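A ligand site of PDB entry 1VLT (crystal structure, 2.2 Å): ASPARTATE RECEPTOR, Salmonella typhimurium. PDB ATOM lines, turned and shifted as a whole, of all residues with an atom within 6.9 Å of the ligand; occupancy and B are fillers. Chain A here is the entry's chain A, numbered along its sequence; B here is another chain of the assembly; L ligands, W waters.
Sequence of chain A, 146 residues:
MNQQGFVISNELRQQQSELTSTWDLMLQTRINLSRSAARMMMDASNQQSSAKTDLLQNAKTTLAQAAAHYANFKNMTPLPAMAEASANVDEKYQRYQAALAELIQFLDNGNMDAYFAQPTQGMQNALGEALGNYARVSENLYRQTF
Water W3 lies within hydrogen-bond range of O3 of the ligand (2.8 Å), OH of Tyr 115 (2.9 Å) and OG of Ser 34 of chain A (3.0 Å).
Water W2 lies within hydrogen-bond range of the side-chain hydroxyl (OH) of Tyr 115, an oxygen (O1) of the ligand and the backbone carbonyl oxygen (O) of Arg 30.
Water W1 lies within hydrogen-bond range of O of Phe 116, O of Gln 118 and N1 of the ligand.
The backbone carbonyl oxygen (O) of Gln 118 lies within hydrogen-bond range of a nitrogen (N1) of the ligand, at 2.9 Å.
NE of Arg 35 of chain B lies within salt-bridge range of O4 of the ligand, 3.3 Å away.
O2 of the ligand is in salt-bridge range of NH2 of Arg 39 of chain B.
The backbone carbonyl oxygen (O) of Tyr 115 is in hydrogen-bond range of a nitrogen (N1) of the ligand (3.0 Å).
The side-chain hydroxyl of Thr 120 lies within hydrogen-bond range of a nitrogen (N1) of the ligand (3.0 Å).
NH1 of Arg 30 is in salt-bridge range of O4 of the ligand (2.7 Å).
Residues that only touch the ligand: Phe 116 (3.6 Å).
Hydrophobic or aromatic side chains within 4 Å of the ligand: Tyr 115 and Phe 116.
Within 4 Å of the ligand: Arg 30, Tyr 115, Phe 116, Gln 118, Thr 120, Arg 35 of chain B and Arg 39 of chain B.
The nearest printed residue that does not touch the ligand is Leu 103 (4.05 Å).
The side-chain hydroxyl of Thr 120 sits at hydrogen-bond distance from the side-chain amide oxygen of Gln 118 (2.8 Å).
The backbone NH (N) of Ser 34 of chain A sits close to the side-chain hydroxyl (OH) of Tyr 115 (3.4 Å).
O of Arg 39 of chain B lies close to O of Ser 49 of chain B (2.6 Å).
NH2 of Arg 30 lies close to NE2 of Gln 121, 2.4 Å away.
The guanidinium group (NH1) of Arg 39 of chain B is in hydrogen-bond range of the backbone carbonyl oxygen (O) of Arg 35 of chain B (3.4 Å).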
ATOM      1  N   ARG A  30       4.883 -16.722 -11.669  1.00  0.00           N
ATOM      2  CA  ARG A  30       5.426 -16.929 -13.002  1.00  0.00           C
ATOM      3  C   ARG A  30       5.908 -18.366 -13.163  1.00  0.00           C
ATOM      4  O   ARG A  30       5.614 -18.995 -14.187  1.00  0.00           O
ATOM      5  CB  ARG A  30       6.540 -15.936 -13.343  1.00  0.00           C
ATOM      6  CG  ARG A  30       7.061 -16.116 -14.761  1.00  0.00           C
ATOM      7  CD  ARG A  30       7.173 -14.793 -15.563  1.00  0.00           C
ATOM      8  NE  ARG A  30       8.537 -14.303 -15.590  1.00  0.00           N
ATOM      9  CZ  ARG A  30       9.287 -14.138 -16.688  1.00  0.00           C
ATOM     10  NH1 ARG A  30       8.812 -14.359 -17.896  1.00  0.00           N
ATOM     11  NH2 ARG A  30      10.530 -13.695 -16.564  1.00  0.00           N
ATOM     12  N   LEU A  33       2.859 -20.763 -13.433  1.00  0.00           N
ATOM     13  CA  LEU A  33       2.267 -20.648 -14.755  1.00  0.00           C
ATOM     14  C   LEU A  33       3.094 -21.360 -15.817  1.00  0.00           C
ATOM     15  O   LEU A  33       2.562 -22.103 -16.645  1.00  0.00           O
ATOM     16  CB  LEU A  33       2.097 -19.180 -15.149  1.00  0.00           C
ATOM     17  CG  LEU A  33       0.892 -18.478 -14.518  1.00  0.00           C
ATOM     18  CD1 LEU A  33       0.779 -17.106 -15.100  1.00  0.00           C
ATOM     19  CD2 LEU A  33      -0.376 -19.282 -14.775  1.00  0.00           C
ATOM     20  N   SER A  34       4.402 -21.146 -15.784  1.00  0.00           N
ATOM     21  CA  SER A  34       5.286 -21.749 -16.747  1.00  0.00           C
ATOM     22  C   SER A  34       5.227 -23.263 -16.660  1.00  0.00           C
ATOM     23  O   SER A  34       5.139 -23.947 -17.657  1.00  0.00           O
ATOM     24  CB  SER A  34       6.698 -21.247 -16.520  1.00  0.00           C
ATOM     25  OG  SER A  34       7.536 -21.700 -17.554  1.00  0.00           O
ATOM     26  N   ALA A  37       1.998 -24.411 -18.388  1.00  0.00           N
ATOM     27  CA  ALA A  37       2.045 -24.299 -19.850  1.00  0.00           C
ATOM     28  C   ALA A  37       2.905 -25.379 -20.492  1.00  0.00           C
ATOM     29  O   ALA A  37       2.650 -25.802 -21.620  1.00  0.00           O
ATOM     30  CB  ALA A  37       2.540 -22.925 -20.267  1.00  0.00           C
ATOM     31  N   LEU A 100       0.656 -10.734 -15.111  1.00  0.00           N
ATOM     32  CA  LEU A 100       0.499 -12.072 -14.556  1.00  0.00           C
ATOM     33  C   LEU A 100      -0.957 -12.572 -14.581  1.00  0.00           C
ATOM     34  O   LEU A 100      -1.215 -13.767 -14.835  1.00  0.00           O
ATOM     35  CB  LEU A 100       1.036 -12.096 -13.120  1.00  0.00           C
ATOM     36  CG  LEU A 100       2.545 -11.897 -13.042  1.00  0.00           C
ATOM     37  CD1 LEU A 100       3.015 -11.952 -11.608  1.00  0.00           C
ATOM     38  CD2 LEU A 100       3.208 -12.985 -13.872  1.00  0.00           C
ATOM     39  N   LEU A 103      -1.849 -13.531 -18.145  1.00  0.00           N
ATOM     40  CA  LEU A 103      -1.287 -14.824 -18.539  1.00  0.00           C
ATOM     41  C   LEU A 103      -2.132 -15.960 -17.977  1.00  0.00           C
ATOM     42  O   LEU A 103      -2.227 -17.004 -18.566  1.00  0.00           O
ATOM     43  CB  LEU A 103       0.171 -14.949 -18.099  1.00  0.00           C
ATOM     44  CG  LEU A 103       1.192 -14.080 -18.848  1.00  0.00           C
ATOM     45  CD1 LEU A 103       2.593 -14.302 -18.274  1.00  0.00           C
ATOM     46  CD2 LEU A 103       1.174 -14.396 -20.330  1.00  0.00           C
ATOM     47  N   ALA A 114      -0.979 -16.078 -27.267  1.00  0.00           N
ATOM     48  CA  ALA A 114      -0.920 -14.910 -26.406  1.00  0.00           C
ATOM     49  C   ALA A 114      -0.056 -15.067 -25.170  1.00  0.00           C
ATOM     50  O   ALA A 114       0.562 -14.103 -24.728  1.00  0.00           O
ATOM     51  CB  ALA A 114      -2.315 -14.500 -26.011  1.00  0.00           C
ATOM     52  N   TYR A 115      -0.013 -16.271 -24.603  1.00  0.00           N
ATOM     53  CA  TYR A 115       0.788 -16.535 -23.414  1.00  0.00           C
ATOM     54  C   TYR A 115       2.280 -16.354 -23.655  1.00  0.00           C
ATOM     55  O   TYR A 115       2.993 -15.795 -22.817  1.00  0.00           O
ATOM     56  CB  TYR A 115       0.535 -17.970 -22.907  1.00  0.00           C
ATOM     57  CG  TYR A 115       1.468 -18.432 -21.806  1.00  0.00           C
ATOM     58  CD1 TYR A 115       1.324 -17.981 -20.484  1.00  0.00           C
ATOM     59  CD2 TYR A 115       2.530 -19.319 -22.079  1.00  0.00           C
ATOM     60  CE1 TYR A 115       2.199 -18.392 -19.476  1.00  0.00           C
ATOM     61  CE2 TYR A 115       3.417 -19.722 -21.074  1.00  0.00           C
ATOM     62  CZ  TYR A 115       3.234 -19.250 -19.784  1.00  0.00           C
ATOM     63  OH  TYR A 115       4.100 -19.642 -18.798  1.00  0.00           O
ATOM     64  N   PHE A 116       2.760 -16.918 -24.754  1.00  0.00           N
ATOM     65  CA  PHE A 116       4.177 -16.845 -25.121  1.00  0.00           C
ATOM     66  C   PHE A 116       4.587 -15.495 -25.731  1.00  0.00           C
ATOM     67  O   PHE A 116       5.726 -15.040 -25.549  1.00  0.00           O
ATOM     68  CB  PHE A 116       4.516 -17.998 -26.074  1.00  0.00           C
ATOM     69  CG  PHE A 116       4.414 -19.363 -25.438  1.00  0.00           C
ATOM     70  CD1 PHE A 116       5.243 -19.725 -24.386  1.00  0.00           C
ATOM     71  CD2 PHE A 116       3.501 -20.287 -25.891  1.00  0.00           C
ATOM     72  CE1 PHE A 116       5.162 -21.002 -23.784  1.00  0.00           C
ATOM     73  CE2 PHE A 116       3.400 -21.565 -25.304  1.00  0.00           C
ATOM     74  CZ  PHE A 116       4.236 -21.921 -24.241  1.00  0.00           C
ATOM     75  N   ALA A 117       3.670 -14.820 -26.407  1.00  0.00           N
ATOM     76  CA  ALA A 117       4.005 -13.541 -27.019  1.00  0.00           C
ATOM     77  C   ALA A 117       4.180 -12.397 -26.036  1.00  0.00           C
ATOM     78  O   ALA A 117       5.010 -11.536 -26.272  1.00  0.00           O
ATOM     79  CB  ALA A 117       2.996 -13.177 -28.097  1.00  0.00           C
ATOM     80  N   GLN A 118       3.426 -12.399 -24.942  1.00  0.00           N
ATOM     81  CA  GLN A 118       3.521 -11.315 -23.954  1.00  0.00           C
ATOM     82  C   GLN A 118       4.921 -11.069 -23.441  1.00  0.00           C
ATOM     83  O   GLN A 118       5.594 -12.012 -23.022  1.00  0.00           O
ATOM     84  CB  GLN A 118       2.614 -11.570 -22.752  1.00  0.00           C
ATOM     85  CG  GLN A 118       2.567 -10.370 -21.823  1.00  0.00           C
ATOM     86  CD  GLN A 118       2.236 -10.709 -20.402  1.00  0.00           C
ATOM     87  OE1 GLN A 118       3.134 -10.912 -19.585  1.00  0.00           O
ATOM     88  NE2 GLN A 118       0.955 -10.744 -20.078  1.00  0.00           N
ATOM     89  N   PRO A 119       5.362  -9.791 -23.403  1.00  0.00           N
ATOM     90  CA  PRO A 119       6.690  -9.381 -22.930  1.00  0.00           C
ATOM     91  C   PRO A 119       6.773  -9.304 -21.398  1.00  0.00           C
ATOM     92  O   PRO A 119       7.111  -8.265 -20.817  1.00  0.00           O
ATOM     93  CB  PRO A 119       6.891  -8.022 -23.596  1.00  0.00           C
ATOM     94  CG  PRO A 119       5.500  -7.463 -23.620  1.00  0.00           C
ATOM     95  CD  PRO A 119       4.666  -8.660 -24.045  1.00  0.00           C
ATOM     96  N   THR A 120       6.534 -10.439 -20.754  1.00  0.00           N
ATOM     97  CA  THR A 120       6.536 -10.583 -19.318  1.00  0.00           C
ATOM     98  C   THR A 120       7.837 -10.138 -18.626  1.00  0.00           C
ATOM     99  O   THR A 120       7.825  -9.339 -17.698  1.00  0.00           O
ATOM    100  CB  THR A 120       6.266 -12.076 -18.958  1.00  0.00           C
ATOM    101  OG1 THR A 120       5.297 -12.609 -19.857  1.00  0.00           O
ATOM    102  CG2 THR A 120       5.773 -12.223 -17.519  1.00  0.00           C
ATOM    103  N   GLN A 121       8.960 -10.693 -19.071  1.00  0.00           N
ATOM    104  CA  GLN A 121      10.275 -10.416 -18.514  1.00  0.00           C
ATOM    105  C   GLN A 121      10.589  -8.936 -18.459  1.00  0.00           C
ATOM    106  O   GLN A 121      11.204  -8.476 -17.514  1.00  0.00           O
ATOM    107  CB  GLN A 121      11.355 -11.125 -19.311  1.00  0.00           C
ATOM    108  CG  GLN A 121      12.677 -11.058 -18.651  1.00  0.00           C
ATOM    109  CD  GLN A 121      12.767 -11.978 -17.454  1.00  0.00           C
ATOM    110  OE1 GLN A 121      12.989 -11.555 -16.322  1.00  0.00           O
ATOM    111  NE2 GLN A 121      12.633 -13.270 -17.706  1.00  0.00           N
ATOM    112  N   ILE B  31      12.885 -20.133 -13.737  1.00  0.00           N
ATOM    113  CA  ILE B  31      11.915 -19.593 -14.692  1.00  0.00           C
ATOM    114  C   ILE B  31      12.444 -19.857 -16.089  1.00  0.00           C
ATOM    115  O   ILE B  31      11.731 -20.381 -16.938  1.00  0.00           O
ATOM    116  CB  ILE B  31      11.694 -18.064 -14.521  1.00  0.00           C
ATOM    117  CG1 ILE B  31      11.080 -17.763 -13.161  1.00  0.00           C
ATOM    118  CG2 ILE B  31      10.771 -17.531 -15.611  1.00  0.00           C
ATOM    119  CD1 ILE B  31      11.089 -16.311 -12.757  1.00  0.00           C
ATOM    120  N   SER B  34      12.250 -23.486 -17.195  1.00  0.00           N
ATOM    121  CA  SER B  34      10.847 -23.737 -17.493  1.00  0.00           C
ATOM    122  C   SER B  34      10.382 -23.150 -18.845  1.00  0.00           C
ATOM    123  O   SER B  34       9.680 -23.836 -19.622  1.00  0.00           O
ATOM    124  CB  SER B  34       9.984 -23.215 -16.346  1.00  0.00           C
ATOM    125  OG  SER B  34      10.408 -23.783 -15.109  1.00  0.00           O
ATOM    126  N   ARG B  35      10.778 -21.914 -19.124  1.00  0.00           N
ATOM    127  CA  ARG B  35      10.399 -21.262 -20.374  1.00  0.00           C
ATOM    128  C   ARG B  35      11.108 -21.977 -21.532  1.00  0.00           C
ATOM    129  O   ARG B  35      10.578 -22.061 -22.644  1.00  0.00           O
ATOM    130  CB  ARG B  35      10.750 -19.766 -20.344  1.00  0.00           C
ATOM    131  CG  ARG B  35       9.997 -18.963 -19.271  1.00  0.00           C
ATOM    132  CD  ARG B  35      10.342 -17.486 -19.342  1.00  0.00           C
ATOM    133  NE  ARG B  35      10.007 -16.934 -20.644  1.00  0.00           N
ATOM    134  CZ  ARG B  35      10.646 -15.917 -21.232  1.00  0.00           C
ATOM    135  NH1 ARG B  35      11.657 -15.305 -20.645  1.00  0.00           N
ATOM    136  NH2 ARG B  35      10.294 -15.537 -22.463  1.00  0.00           N
ATOM    137  N   SER B  36      12.300 -22.502 -21.260  1.00  0.00           N
ATOM    138  CA  SER B  36      13.067 -23.242 -22.254  1.00  0.00           C
ATOM    139  C   SER B  36      12.282 -24.540 -22.542  1.00  0.00           C
ATOM    140  O   SER B  36      11.837 -24.783 -23.655  1.00  0.00           O
ATOM    141  CB  SER B  36      14.462 -23.532 -21.704  1.00  0.00           C
ATOM    142  OG  SER B  36      15.106 -24.522 -22.462  1.00  0.00           O
ATOM    143  N   ALA B  38       9.150 -25.491 -21.908  1.00  0.00           N
ATOM    144  CA  ALA B  38       7.856 -25.301 -22.551  1.00  0.00           C
ATOM    145  C   ALA B  38       8.016 -25.089 -24.055  1.00  0.00           C
ATOM    146  O   ALA B  38       7.191 -25.558 -24.835  1.00  0.00           O
ATOM    147  CB  ALA B  38       7.118 -24.123 -21.956  1.00  0.00           C
ATOM    148  N   ARG B  39       9.071 -24.406 -24.466  1.00  0.00           N
ATOM    149  CA  ARG B  39       9.296 -24.150 -25.878  1.00  0.00           C
ATOM    150  C   ARG B  39       9.873 -25.341 -26.598  1.00  0.00           C
ATOM    151  O   ARG B  39       9.837 -25.397 -27.822  1.00  0.00           O
ATOM    152  CB  ARG B  39      10.174 -22.943 -26.093  1.00  0.00           C
ATOM    153  CG  ARG B  39       9.426 -21.641 -25.933  1.00  0.00           C
ATOM    154  CD  ARG B  39      10.406 -20.519 -25.830  1.00  0.00           C
ATOM    155  NE  ARG B  39       9.768 -19.217 -25.882  1.00  0.00           N
ATOM    156  CZ  ARG B  39       9.136 -18.644 -24.882  1.00  0.00           C
ATOM    157  NH1 ARG B  39       9.033 -19.264 -23.716  1.00  0.00           N
ATOM    158  NH2 ARG B  39       8.614 -17.434 -25.043  1.00  0.00           N
ATOM    159  N   SER B  49       6.253 -24.652 -28.684  1.00  0.00           N
ATOM    160  CA  SER B  49       6.485 -23.299 -29.177  1.00  0.00           C
ATOM    161  C   SER B  49       7.915 -23.043 -29.704  1.00  0.00           C
ATOM    162  O   SER B  49       8.743 -23.955 -29.748  1.00  0.00           O
ATOM    163  CB  SER B  49       6.066 -22.260 -28.122  1.00  0.00           C
ATOM    164  OG  SER B  49       6.526 -22.613 -26.839  1.00  0.00           O
ATOM    165  N   LEU B  55      17.295 -19.524 -24.008  1.00  0.00           N
ATOM    166  CA  LEU B  55      16.728 -19.498 -22.652  1.00  0.00           C
ATOM    167  C   LEU B  55      17.477 -20.415 -21.700  1.00  0.00           C
ATOM    168  O   LEU B  55      17.765 -20.033 -20.582  1.00  0.00           O
ATOM    169  CB  LEU B  55      15.208 -19.762 -22.668  1.00  0.00           C
ATOM    170  CG  LEU B  55      14.333 -18.557 -23.080  1.00  0.00           C
ATOM    171  CD1 LEU B  55      12.913 -18.962 -23.432  1.00  0.00           C
ATOM    172  CD2 LEU B  55      14.322 -17.506 -21.979  1.00  0.00           C
HETATM  173  N1  LIG L   1       5.674 -14.673 -21.952  1.00  0.00           N
HETATM  174  C1  LIG L   1       5.443 -15.618 -20.828  1.00  0.00           C
HETATM  175  C2  LIG L   1       6.557 -15.404 -19.834  1.00  0.00           C
HETATM  176  O1  LIG L   1       6.381 -15.786 -18.654  1.00  0.00           O
HETATM  177  C3  LIG L   1       5.406 -17.073 -21.315  1.00  0.00           C
HETATM  178  C4  LIG L   1       6.734 -17.524 -21.908  1.00  0.00           C
HETATM  179  O2  LIG L   1       7.234 -16.804 -22.784  1.00  0.00           O
HETATM  180  O3  LIG L   1       7.251 -18.593 -21.507  1.00  0.00           O
HETATM  181  O4  LIG L   1       7.574 -14.795 -20.244  1.00  0.00           O
HETATM  182  O   HOH W   1       7.768 -13.717 -24.082  1.00  0.00           O
HETATM  183  O   HOH W   2       4.750 -17.597 -16.978  1.00  0.00           O
HETATM  184  O   HOH W   3       6.335 -20.921 -20.159  1.00  0.00           O
